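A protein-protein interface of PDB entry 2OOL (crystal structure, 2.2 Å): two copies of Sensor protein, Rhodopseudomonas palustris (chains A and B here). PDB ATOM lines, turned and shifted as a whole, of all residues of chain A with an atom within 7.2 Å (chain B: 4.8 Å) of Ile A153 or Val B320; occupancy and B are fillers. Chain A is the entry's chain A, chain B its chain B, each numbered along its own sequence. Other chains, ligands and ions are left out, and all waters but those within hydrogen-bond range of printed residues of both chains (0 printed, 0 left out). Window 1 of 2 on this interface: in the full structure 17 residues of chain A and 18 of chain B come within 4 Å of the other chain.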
ATOM      1  N   ARG A 147     -25.620 -24.499   4.224  1.00  0.00           N
ATOM      2  CA  ARG A 147     -25.231 -24.565   5.631  1.00  0.00           C
ATOM      3  C   ARG A 147     -23.729 -24.378   5.804  1.00  0.00           C
ATOM      4  O   ARG A 147     -23.314 -23.584   6.639  1.00  0.00           O
ATOM      5  CB  ARG A 147     -25.689 -25.913   6.239  1.00  0.00           C
ATOM      6  CG  ARG A 147     -25.210 -26.198   7.632  1.00  0.00           C
ATOM      7  CD  ARG A 147     -25.729 -27.541   8.060  1.00  0.00           C
ATOM      8  NE  ARG A 147     -25.059 -28.639   7.364  1.00  0.00           N
ATOM      9  CZ  ARG A 147     -25.608 -29.830   7.093  1.00  0.00           C
ATOM     10  NH1 ARG A 147     -26.866 -30.110   7.426  1.00  0.00           N
ATOM     11  NH2 ARG A 147     -24.891 -30.756   6.464  1.00  0.00           N
ATOM     12  N   SER A 148     -22.928 -25.067   4.984  1.00  0.00           N
ATOM     13  CA  SER A 148     -21.466 -24.934   5.087  1.00  0.00           C
ATOM     14  C   SER A 148     -21.007 -23.510   4.756  1.00  0.00           C
ATOM     15  O   SER A 148     -20.198 -22.948   5.481  1.00  0.00           O
ATOM     16  CB  SER A 148     -20.688 -25.988   4.251  1.00  0.00           C
ATOM     17  OG  SER A 148     -20.823 -25.776   2.864  1.00  0.00           O
ATOM     18  N   VAL A 149     -21.536 -22.906   3.687  1.00  0.00           N
ATOM     19  CA  VAL A 149     -21.203 -21.497   3.380  1.00  0.00           C
ATOM     20  C   VAL A 149     -21.562 -20.548   4.562  1.00  0.00           C
ATOM     21  O   VAL A 149     -20.761 -19.714   4.978  1.00  0.00           O
ATOM     22  CB  VAL A 149     -21.828 -21.015   2.057  1.00  0.00           C
ATOM     23  CG1 VAL A 149     -21.655 -19.495   1.911  1.00  0.00           C
ATOM     24  CG2 VAL A 149     -21.211 -21.751   0.856  1.00  0.00           C
ATOM     25  N   ARG A 150     -22.732 -20.742   5.154  1.00  0.00           N
ATOM     26  CA  ARG A 150     -23.172 -19.942   6.302  1.00  0.00           C
ATOM     27  C   ARG A 150     -22.243 -20.064   7.544  1.00  0.00           C
ATOM     28  O   ARG A 150     -21.872 -19.043   8.154  1.00  0.00           O
ATOM     29  CB  ARG A 150     -24.630 -20.288   6.659  1.00  0.00           C
ATOM     30  CG  ARG A 150     -25.132 -19.576   7.919  1.00  0.00           C
ATOM     31  CD  ARG A 150     -26.512 -20.048   8.378  1.00  0.00           C
ATOM     32  NE  ARG A 150     -26.496 -21.370   9.015  1.00  0.00           N
ATOM     33  CZ  ARG A 150     -26.057 -21.622  10.244  1.00  0.00           C
ATOM     34  NH1 ARG A 150     -26.101 -22.868  10.704  1.00  0.00           N
ATOM     35  NH2 ARG A 150     -25.560 -20.653  11.014  1.00  0.00           N
ATOM     36  N   VAL A 151     -21.879 -21.286   7.936  1.00  0.00           N
ATOM     37  CA  VAL A 151     -21.053 -21.430   9.135  1.00  0.00           C
ATOM     38  C   VAL A 151     -19.629 -20.915   8.852  1.00  0.00           C
ATOM     39  O   VAL A 151     -19.036 -20.277   9.692  1.00  0.00           O
ATOM     40  CB  VAL A 151     -21.137 -22.854   9.858  1.00  0.00           C
ATOM     41  CG1 VAL A 151     -22.488 -23.551   9.634  1.00  0.00           C
ATOM     42  CG2 VAL A 151     -19.938 -23.781   9.552  1.00  0.00           C
ATOM     43  N   ALA A 152     -19.113 -21.137   7.649  1.00  0.00           N
ATOM     44  CA  ALA A 152     -17.820 -20.549   7.214  1.00  0.00           C
ATOM     45  C   ALA A 152     -17.791 -19.005   7.278  1.00  0.00           C
ATOM     46  O   ALA A 152     -16.842 -18.441   7.794  1.00  0.00           O
ATOM     47  CB  ALA A 152     -17.468 -21.021   5.815  1.00  0.00           C
ATOM     48  N   ILE A 153     -18.806 -18.335   6.739  1.00  0.00           N
ATOM     49  CA  ILE A 153     -18.877 -16.857   6.777  1.00  0.00           C
ATOM     50  C   ILE A 153     -18.846 -16.351   8.224  1.00  0.00           C
ATOM     51  O   ILE A 153     -18.159 -15.399   8.557  1.00  0.00           O
ATOM     52  CB  ILE A 153     -20.193 -16.316   6.155  1.00  0.00           C
ATOM     53  CG1 ILE A 153     -20.187 -16.421   4.634  1.00  0.00           C
ATOM     54  CG2 ILE A 153     -20.440 -14.844   6.561  1.00  0.00           C
ATOM     55  CD1 ILE A 153     -21.541 -15.993   3.991  1.00  0.00           C
ATOM     56  N   ARG A 154     -19.644 -16.978   9.065  1.00  0.00           N
ATOM     57  CA  ARG A 154     -19.659 -16.657  10.482  1.00  0.00           C
ATOM     58  C   ARG A 154     -18.294 -16.880  11.183  1.00  0.00           C
ATOM     59  O   ARG A 154     -17.897 -16.084  12.043  1.00  0.00           O
ATOM     60  CB  ARG A 154     -20.749 -17.492  11.145  1.00  0.00           C
ATOM     61  CG  ARG A 154     -21.013 -17.166  12.582  1.00  0.00           C
ATOM     62  CD  ARG A 154     -21.818 -18.300  13.170  1.00  0.00           C
ATOM     63  NE  ARG A 154     -20.960 -19.398  13.617  1.00  0.00           N
ATOM     64  CZ  ARG A 154     -21.345 -20.672  13.734  1.00  0.00           C
ATOM     65  NH1 ARG A 154     -22.583 -21.043  13.387  1.00  0.00           N
ATOM     66  NH2 ARG A 154     -20.484 -21.590  14.199  1.00  0.00           N
ATOM     67  N   ARG A 155     -17.589 -17.945  10.810  1.00  0.00           N
ATOM     68  CA  ARG A 155     -16.294 -18.260  11.413  1.00  0.00           C
ATOM     69  C   ARG A 155     -15.238 -17.283  10.946  1.00  0.00           C
ATOM     70  O   ARG A 155     -14.403 -16.826  11.724  1.00  0.00           O
ATOM     71  CB  ARG A 155     -15.841 -19.673  11.061  1.00  0.00           C
ATOM     72  CG  ARG A 155     -16.437 -20.720  11.960  1.00  0.00           C
ATOM     73  CD  ARG A 155     -16.303 -22.135  11.390  1.00  0.00           C
ATOM     74  NE  ARG A 155     -17.077 -23.081  12.211  1.00  0.00           N
ATOM     75  CZ  ARG A 155     -17.122 -24.405  12.034  1.00  0.00           C
ATOM     76  NH1 ARG A 155     -16.421 -24.997  11.057  1.00  0.00           N
ATOM     77  NH2 ARG A 155     -17.883 -25.139  12.834  1.00  0.00           N
ATOM     78  N   LEU A 156     -15.280 -16.981   9.660  1.00  0.00           N
ATOM     79  CA  LEU A 156     -14.363 -16.036   9.071  1.00  0.00           C
ATOM     80  C   LEU A 156     -14.485 -14.724   9.823  1.00  0.00           C
ATOM     81  O   LEU A 156     -13.489 -14.093  10.127  1.00  0.00           O
ATOM     82  CB  LEU A 156     -14.714 -15.845   7.590  1.00  0.00           C
ATOM     83  CG  LEU A 156     -13.653 -16.001   6.508  1.00  0.00           C
ATOM     84  CD1 LEU A 156     -12.579 -16.953   6.829  1.00  0.00           C
ATOM     85  CD2 LEU A 156     -14.342 -16.413   5.152  1.00  0.00           C
ATOM     86  N   GLN A 157     -15.709 -14.356  10.188  1.00  0.00           N
ATOM     87  CA  GLN A 157     -15.969 -13.061  10.808  1.00  0.00           C
ATOM     88  C   GLN A 157     -15.527 -12.917  12.261  1.00  0.00           C
ATOM     89  O   GLN A 157     -15.442 -11.788  12.747  1.00  0.00           O
ATOM     90  CB  GLN A 157     -17.449 -12.704  10.690  1.00  0.00           C
ATOM     91  CG  GLN A 157     -17.928 -12.451   9.245  1.00  0.00           C
ATOM     92  CD  GLN A 157     -19.025 -11.418   9.192  1.00  0.00           C
ATOM     93  OE1 GLN A 157     -20.221 -11.753   9.088  1.00  0.00           O
ATOM     94  NE2 GLN A 157     -18.633 -10.142   9.300  1.00  0.00           N
ATOM     95  N   THR A 158     -15.264 -14.033  12.953  1.00  0.00           N
ATOM     96  CA  THR A 158     -14.620 -13.994  14.277  1.00  0.00           C
ATOM     97  C   THR A 158     -13.189 -14.547  14.282  1.00  0.00           C
ATOM     98  O   THR A 158     -12.655 -14.833  15.341  1.00  0.00           O
ATOM     99  CB  THR A 158     -15.452 -14.760  15.352  1.00  0.00           C
ATOM    100  OG1 THR A 158     -15.735 -16.089  14.898  1.00  0.00           O
ATOM    101  CG2 THR A 158     -16.766 -14.009  15.695  1.00  0.00           C
ATOM    102  N   ILE A 168      -9.577 -20.797   7.173  1.00  0.00           N
ATOM    103  CA  ILE A 168     -11.012 -21.010   7.150  1.00  0.00           C
ATOM    104  C   ILE A 168     -11.475 -20.864   5.690  1.00  0.00           C
ATOM    105  O   ILE A 168     -12.181 -21.696   5.187  1.00  0.00           O
ATOM    106  CB  ILE A 168     -11.762 -20.015   8.094  1.00  0.00           C
ATOM    107  CG1 ILE A 168     -11.439 -20.332   9.577  1.00  0.00           C
ATOM    108  CG2 ILE A 168     -13.279 -20.047   7.840  1.00  0.00           C
ATOM    109  CD1 ILE A 168     -11.487 -19.149  10.565  1.00  0.00           C
ATOM    110  N   GLU A 172     -13.006 -24.224   3.486  1.00  0.00           N
ATOM    111  CA  GLU A 172     -14.382 -24.234   2.957  1.00  0.00           C
ATOM    112  C   GLU A 172     -14.419 -24.313   1.429  1.00  0.00           C
ATOM    113  O   GLU A 172     -15.235 -25.018   0.850  1.00  0.00           O
ATOM    114  CB  GLU A 172     -15.172 -23.014   3.421  1.00  0.00           C
ATOM    115  CG  GLU A 172     -16.597 -22.883   2.733  1.00  0.00           C
ATOM    116  CD  GLU A 172     -17.634 -23.861   3.305  1.00  0.00           C
ATOM    117  OE1 GLU A 172     -17.331 -24.569   4.274  1.00  0.00           O
ATOM    118  OE2 GLU A 172     -18.776 -23.899   2.808  1.00  0.00           O
ATOM    119  N   LEU A 316     -18.085 -15.258  -2.953  1.00  0.00           N
ATOM    120  CA  LEU A 316     -18.671 -14.800  -1.695  1.00  0.00           C
ATOM    121  C   LEU A 316     -17.715 -14.998  -0.524  1.00  0.00           C
ATOM    122  O   LEU A 316     -17.487 -14.066   0.274  1.00  0.00           O
ATOM    123  CB  LEU A 316     -19.975 -15.530  -1.410  1.00  0.00           C
ATOM    124  CG  LEU A 316     -20.730 -15.194  -0.129  1.00  0.00           C
ATOM    125  CD1 LEU A 316     -21.060 -13.701   0.008  1.00  0.00           C
ATOM    126  CD2 LEU A 316     -22.002 -16.061  -0.060  1.00  0.00           C
ATOM    127  N   ILE A 317     -17.185 -16.213  -0.412  1.00  0.00           N
ATOM    128  CA  ILE A 317     -16.209 -16.542   0.633  1.00  0.00           C
ATOM    129  C   ILE A 317     -14.999 -15.593   0.592  1.00  0.00           C
ATOM    130  O   ILE A 317     -14.530 -15.095   1.638  1.00  0.00           O
ATOM    131  CB  ILE A 317     -15.812 -18.024   0.549  1.00  0.00           C
ATOM    132  CG1 ILE A 317     -16.941 -18.885   1.151  1.00  0.00           C
ATOM    133  CG2 ILE A 317     -14.499 -18.348   1.320  1.00  0.00           C
ATOM    134  CD1 ILE A 317     -16.940 -20.300   0.679  1.00  0.00           C
ATOM    135  N   VAL A 320     -15.919 -12.055   1.836  1.00  0.00           N
ATOM    136  CA  VAL A 320     -15.961 -11.969   3.315  1.00  0.00           C
ATOM    137  C   VAL A 320     -14.564 -12.000   3.926  1.00  0.00           C
ATOM    138  O   VAL A 320     -14.284 -11.282   4.932  1.00  0.00           O
ATOM    139  CB  VAL A 320     -16.799 -13.102   3.937  1.00  0.00           C
ATOM    140  CG1 VAL A 320     -16.720 -13.096   5.544  1.00  0.00           C
ATOM    141  CG2 VAL A 320     -18.222 -13.018   3.459  1.00  0.00           C
ATOM    142  N   GLN A 324     -12.478  -9.211   6.237  1.00  0.00           N
ATOM    143  CA  GLN A 324     -11.819  -9.559   7.478  1.00  0.00           C
ATOM    144  C   GLN A 324     -10.319  -9.259   7.476  1.00  0.00           C
ATOM    145  O   GLN A 324      -9.743  -8.933   8.518  1.00  0.00           O
ATOM    146  CB  GLN A 324     -12.062 -11.016   7.846  1.00  0.00           C
ATOM    147  CG  GLN A 324     -11.781 -11.326   9.333  1.00  0.00           C
ATOM    148  CD  GLN A 324     -12.818 -10.762  10.318  1.00  0.00           C
ATOM    149  OE1 GLN A 324     -13.757 -10.042   9.948  1.00  0.00           O
ATOM    150  NE2 GLN A 324     -12.661 -11.122  11.570  1.00  0.00           N
ATOM    151  N   ILE B 153     -29.053 -13.548  -2.116  1.00  0.00           N
ATOM    152  CA  ILE B 153     -27.706 -13.326  -1.637  1.00  0.00           C
ATOM    153  C   ILE B 153     -26.907 -12.504  -2.633  1.00  0.00           C
ATOM    154  O   ILE B 153     -26.144 -11.638  -2.214  1.00  0.00           O
ATOM    155  CB  ILE B 153     -26.986 -14.662  -1.331  1.00  0.00           C
ATOM    156  CG1 ILE B 153     -27.540 -15.252  -0.033  1.00  0.00           C
ATOM    157  CG2 ILE B 153     -25.492 -14.448  -1.180  1.00  0.00           C
ATOM    158  CD1 ILE B 153     -27.154 -16.696   0.167  1.00  0.00           C
ATOM    159  N   LEU B 156     -27.928  -8.915  -2.231  1.00  0.00           N
ATOM    160  CA  LEU B 156     -27.289  -8.378  -1.003  1.00  0.00           C
ATOM    161  C   LEU B 156     -25.816  -8.012  -1.198  1.00  0.00           C
ATOM    162  O   LEU B 156     -25.366  -6.984  -0.702  1.00  0.00           O
ATOM    163  CB  LEU B 156     -27.400  -9.365   0.165  1.00  0.00           C
ATOM    164  CG  LEU B 156     -28.730  -9.473   0.923  1.00  0.00           C
ATOM    165  CD1 LEU B 156     -28.706 -10.704   1.851  1.00  0.00           C
ATOM    166  CD2 LEU B 156     -29.078  -8.173   1.693  1.00  0.00           C
ATOM    167  N   LEU B 316     -28.934 -18.047   6.563  1.00  0.00           N
ATOM    168  CA  LEU B 316     -27.876 -17.704   5.590  1.00  0.00           C
ATOM    169  C   LEU B 316     -28.060 -16.265   5.130  1.00  0.00           C
ATOM    170  O   LEU B 316     -27.117 -15.480   5.178  1.00  0.00           O
ATOM    171  CB  LEU B 316     -27.805 -18.668   4.397  1.00  0.00           C
ATOM    172  CG  LEU B 316     -26.828 -18.309   3.237  1.00  0.00           C
ATOM    173  CD1 LEU B 316     -25.404 -18.149   3.759  1.00  0.00           C
ATOM    174  CD2 LEU B 316     -26.858 -19.352   2.111  1.00  0.00           C
ATOM    175  N   ILE B 317     -29.279 -15.912   4.746  1.00  0.00           N
ATOM    176  CA  ILE B 317     -29.587 -14.543   4.357  1.00  0.00           C
ATOM    177  C   ILE B 317     -29.289 -13.578   5.480  1.00  0.00           C
ATOM    178  O   ILE B 317     -28.701 -12.538   5.225  1.00  0.00           O
ATOM    179  CB  ILE B 317     -31.071 -14.366   3.935  1.00  0.00           C
ATOM    180  CG1 ILE B 317     -31.333 -15.092   2.622  1.00  0.00           C
ATOM    181  CG2 ILE B 317     -31.436 -12.891   3.769  1.00  0.00           C
ATOM    182  CD1 ILE B 317     -32.763 -15.492   2.448  1.00  0.00           C
ATOM    183  N   ALA B 318     -29.703 -13.893   6.713  1.00  0.00           N
ATOM    184  CA  ALA B 318     -29.386 -13.017   7.875  1.00  0.00           C
ATOM    185  C   ALA B 318     -27.894 -12.832   8.015  1.00  0.00           C
ATOM    186  O   ALA B 318     -27.410 -11.724   8.256  1.00  0.00           O
ATOM    187  CB  ALA B 318     -29.976 -13.558   9.190  1.00  0.00           C
ATOM    188  N   GLN B 319     -27.165 -13.921   7.826  1.00  0.00           N
ATOM    189  CA  GLN B 319     -25.699 -13.917   7.967  1.00  0.00           C
ATOM    190  C   GLN B 319     -24.966 -13.083   6.896  1.00  0.00           C
ATOM    191  O   GLN B 319     -23.948 -12.450   7.191  1.00  0.00           O
ATOM    192  CB  GLN B 319     -25.172 -15.352   7.945  1.00  0.00           C
ATOM    193  CG  GLN B 319     -23.727 -15.493   8.416  1.00  0.00           C
ATOM    194  CD  GLN B 319     -23.599 -15.306   9.917  1.00  0.00           C
ATOM    195  OE1 GLN B 319     -24.417 -15.809  10.686  1.00  0.00           O
ATOM    196  NE2 GLN B 319     -22.590 -14.564  10.335  1.00  0.00           N
ATOM    197  N   VAL B 320     -25.455 -13.124   5.656  1.00  0.00           N
ATOM    198  CA  VAL B 320     -24.934 -12.246   4.587  1.00  0.00           C
ATOM    199  C   VAL B 320     -25.342 -10.777   4.821  1.00  0.00           C
ATOM    200  O   VAL B 320     -24.540  -9.873   4.611  1.00  0.00           O
ATOM    201  CB  VAL B 320     -25.331 -12.741   3.161  1.00  0.00           C
ATOM    202  CG1 VAL B 320     -24.910 -11.717   2.052  1.00  0.00           C
ATOM    203  CG2 VAL B 320     -24.674 -14.103   2.890  1.00  0.00           C
ATOM    204  N   LEU B 321     -26.565 -10.544   5.283  1.00  0.00           N
ATOM    205  CA  LEU B 321     -26.971  -9.195   5.646  1.00  0.00           C
ATOM    206  C   LEU B 321     -26.094  -8.635   6.770  1.00  0.00           C
ATOM    207  O   LEU B 321     -25.754  -7.434   6.769  1.00  0.00           O
ATOM    208  CB  LEU B 321     -28.421  -9.183   6.085  1.00  0.00           C
ATOM    209  CG  LEU B 321     -28.869  -7.862   6.721  1.00  0.00           C
ATOM    210  CD1 LEU B 321     -28.851  -6.738   5.678  1.00  0.00           C
ATOM    211  CD2 LEU B 321     -30.242  -8.009   7.349  1.00  0.00           C
ATOM    212  N   THR B 322     -25.743  -9.505   7.727  1.00  0.00           N
ATOM    213  CA  THR B 322     -24.948  -9.119   8.893  1.00  0.00           C
ATOM    214  C   THR B 322     -23.594  -8.572   8.462  1.00  0.00           C
ATOM    215  O   THR B 322     -23.188  -7.464   8.861  1.00  0.00           O
ATOM    216  CB  THR B 322     -24.711 -10.328   9.853  1.00  0.00           C
ATOM    217  OG1 THR B 322     -25.970 -10.866  10.277  1.00  0.00           O
ATOM    218  CG2 THR B 322     -23.890  -9.921  11.070  1.00  0.00           C
ATOM    219  N   TRP B 323     -22.898  -9.360   7.654  1.00  0.00           N
ATOM    220  CA  TRP B 323     -21.625  -8.946   7.076  1.00  0.00           C
ATOM    221  C   TRP B 323     -21.792  -7.593   6.364  1.00  0.00           C
ATOM    222  O   TRP B 323     -20.980  -6.693   6.546  1.00  0.00           O
ATOM    223  CB  TRP B 323     -21.079 -10.041   6.132  1.00  0.00           C
ATOM    224  CG  TRP B 323     -20.080  -9.582   5.067  1.00  0.00           C
ATOM    225  CD1 TRP B 323     -18.864  -9.014   5.276  1.00  0.00           C
ATOM    226  CD2 TRP B 323     -20.234  -9.673   3.643  1.00  0.00           C
ATOM    227  NE1 TRP B 323     -18.254  -8.735   4.076  1.00  0.00           N
ATOM    228  CE2 TRP B 323     -19.074  -9.135   3.060  1.00  0.00           C
ATOM    229  CE3 TRP B 323     -21.246 -10.146   2.808  1.00  0.00           C
ATOM    230  CZ2 TRP B 323     -18.891  -9.080   1.697  1.00  0.00           C
ATOM    231  CZ3 TRP B 323     -21.058 -10.091   1.445  1.00  0.00           C
ATOM    232  CH2 TRP B 323     -19.902  -9.550   0.905  1.00  0.00           C
ATOM    233  N   GLN B 324     -22.870  -7.448   5.607  1.00  0.00           N
ATOM    234  CA  GLN B 324     -23.055  -6.259   4.763  1.00  0.00           C
ATOM    235  C   GLN B 324     -23.322  -5.009   5.597  1.00  0.00           C
ATOM    236  O   GLN B 324     -22.841  -3.938   5.269  1.00  0.00           O
ATOM    237  CB  GLN B 324     -24.166  -6.464   3.725  1.00  0.00           C
ATOM    238  CG  GLN B 324     -23.877  -5.770   2.414  1.00  0.00           C
ATOM    239  CD  GLN B 324     -22.780  -6.447   1.633  1.00  0.00           C
ATOM    240  OE1 GLN B 324     -21.797  -5.825   1.269  1.00  0.00           O
ATOM    241  NE2 GLN B 324     -22.941  -7.741   1.387  1.00  0.00           N
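Ile A153 touches Val B320, but with the chains exchanged Val A320 does not touch Ile B153 (8.7 Å).
Among the printed residues, pairs that only touch across the chains: Gln A157 with Trp B323, Arg A154 with Gln B319, Arg A150 with Leu B316, Ile A153 with Val B320, Ile A153 with Gln B319, Gln A157 with Gln B319, Leu A316 with Trp B323 and Val A320 with Trp B323.
Of the 11 printed residues of chain B, 4 touch a printed residue of chain A. Hydrophobic or aromatic side chains of chain B within 4 Å of the printed part of chain A: Leu B316, Val B320 and Trp B323. Of the 18 printed residues of chain A, 6 touch a printed residue of chain B.
The backbone carbonyl oxygen (O) of Gln A157 is in hydrogen-bond range of the side-chain amide nitrogen (NE2) of Gln A324, at 3.1 Å.
Ile A153 touches just these residues of chain B: Gln B319 (3.8 Å) and Val B320 (3.8 Å). Val B320 touches just one residue of chain A: Ile A153. Printed residues of chain A within 4 Å of Gln B319: Ile A153 (3.8 Å), Arg A154 (3.6 Å) and Gln A157 (3.9 Å). Printed residues of chain A within 4 Å of Leu B316: Arg A150 (3.6 Å). Printed residues of chain B within 4 Å of Gln A157: Gln B319 and Trp B323. Of the printed residues of chain B, Leu A316 touches Trp B323 (3.9 Å). Thr B322 touches none of the printed residues of chain A. The nearest residue of chain A that does not touch Val B320 is Leu A316 (4.4 Å). The nearest printed residue of chain B that does not touch Gln A157 is Thr B322 (4.6 Å).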
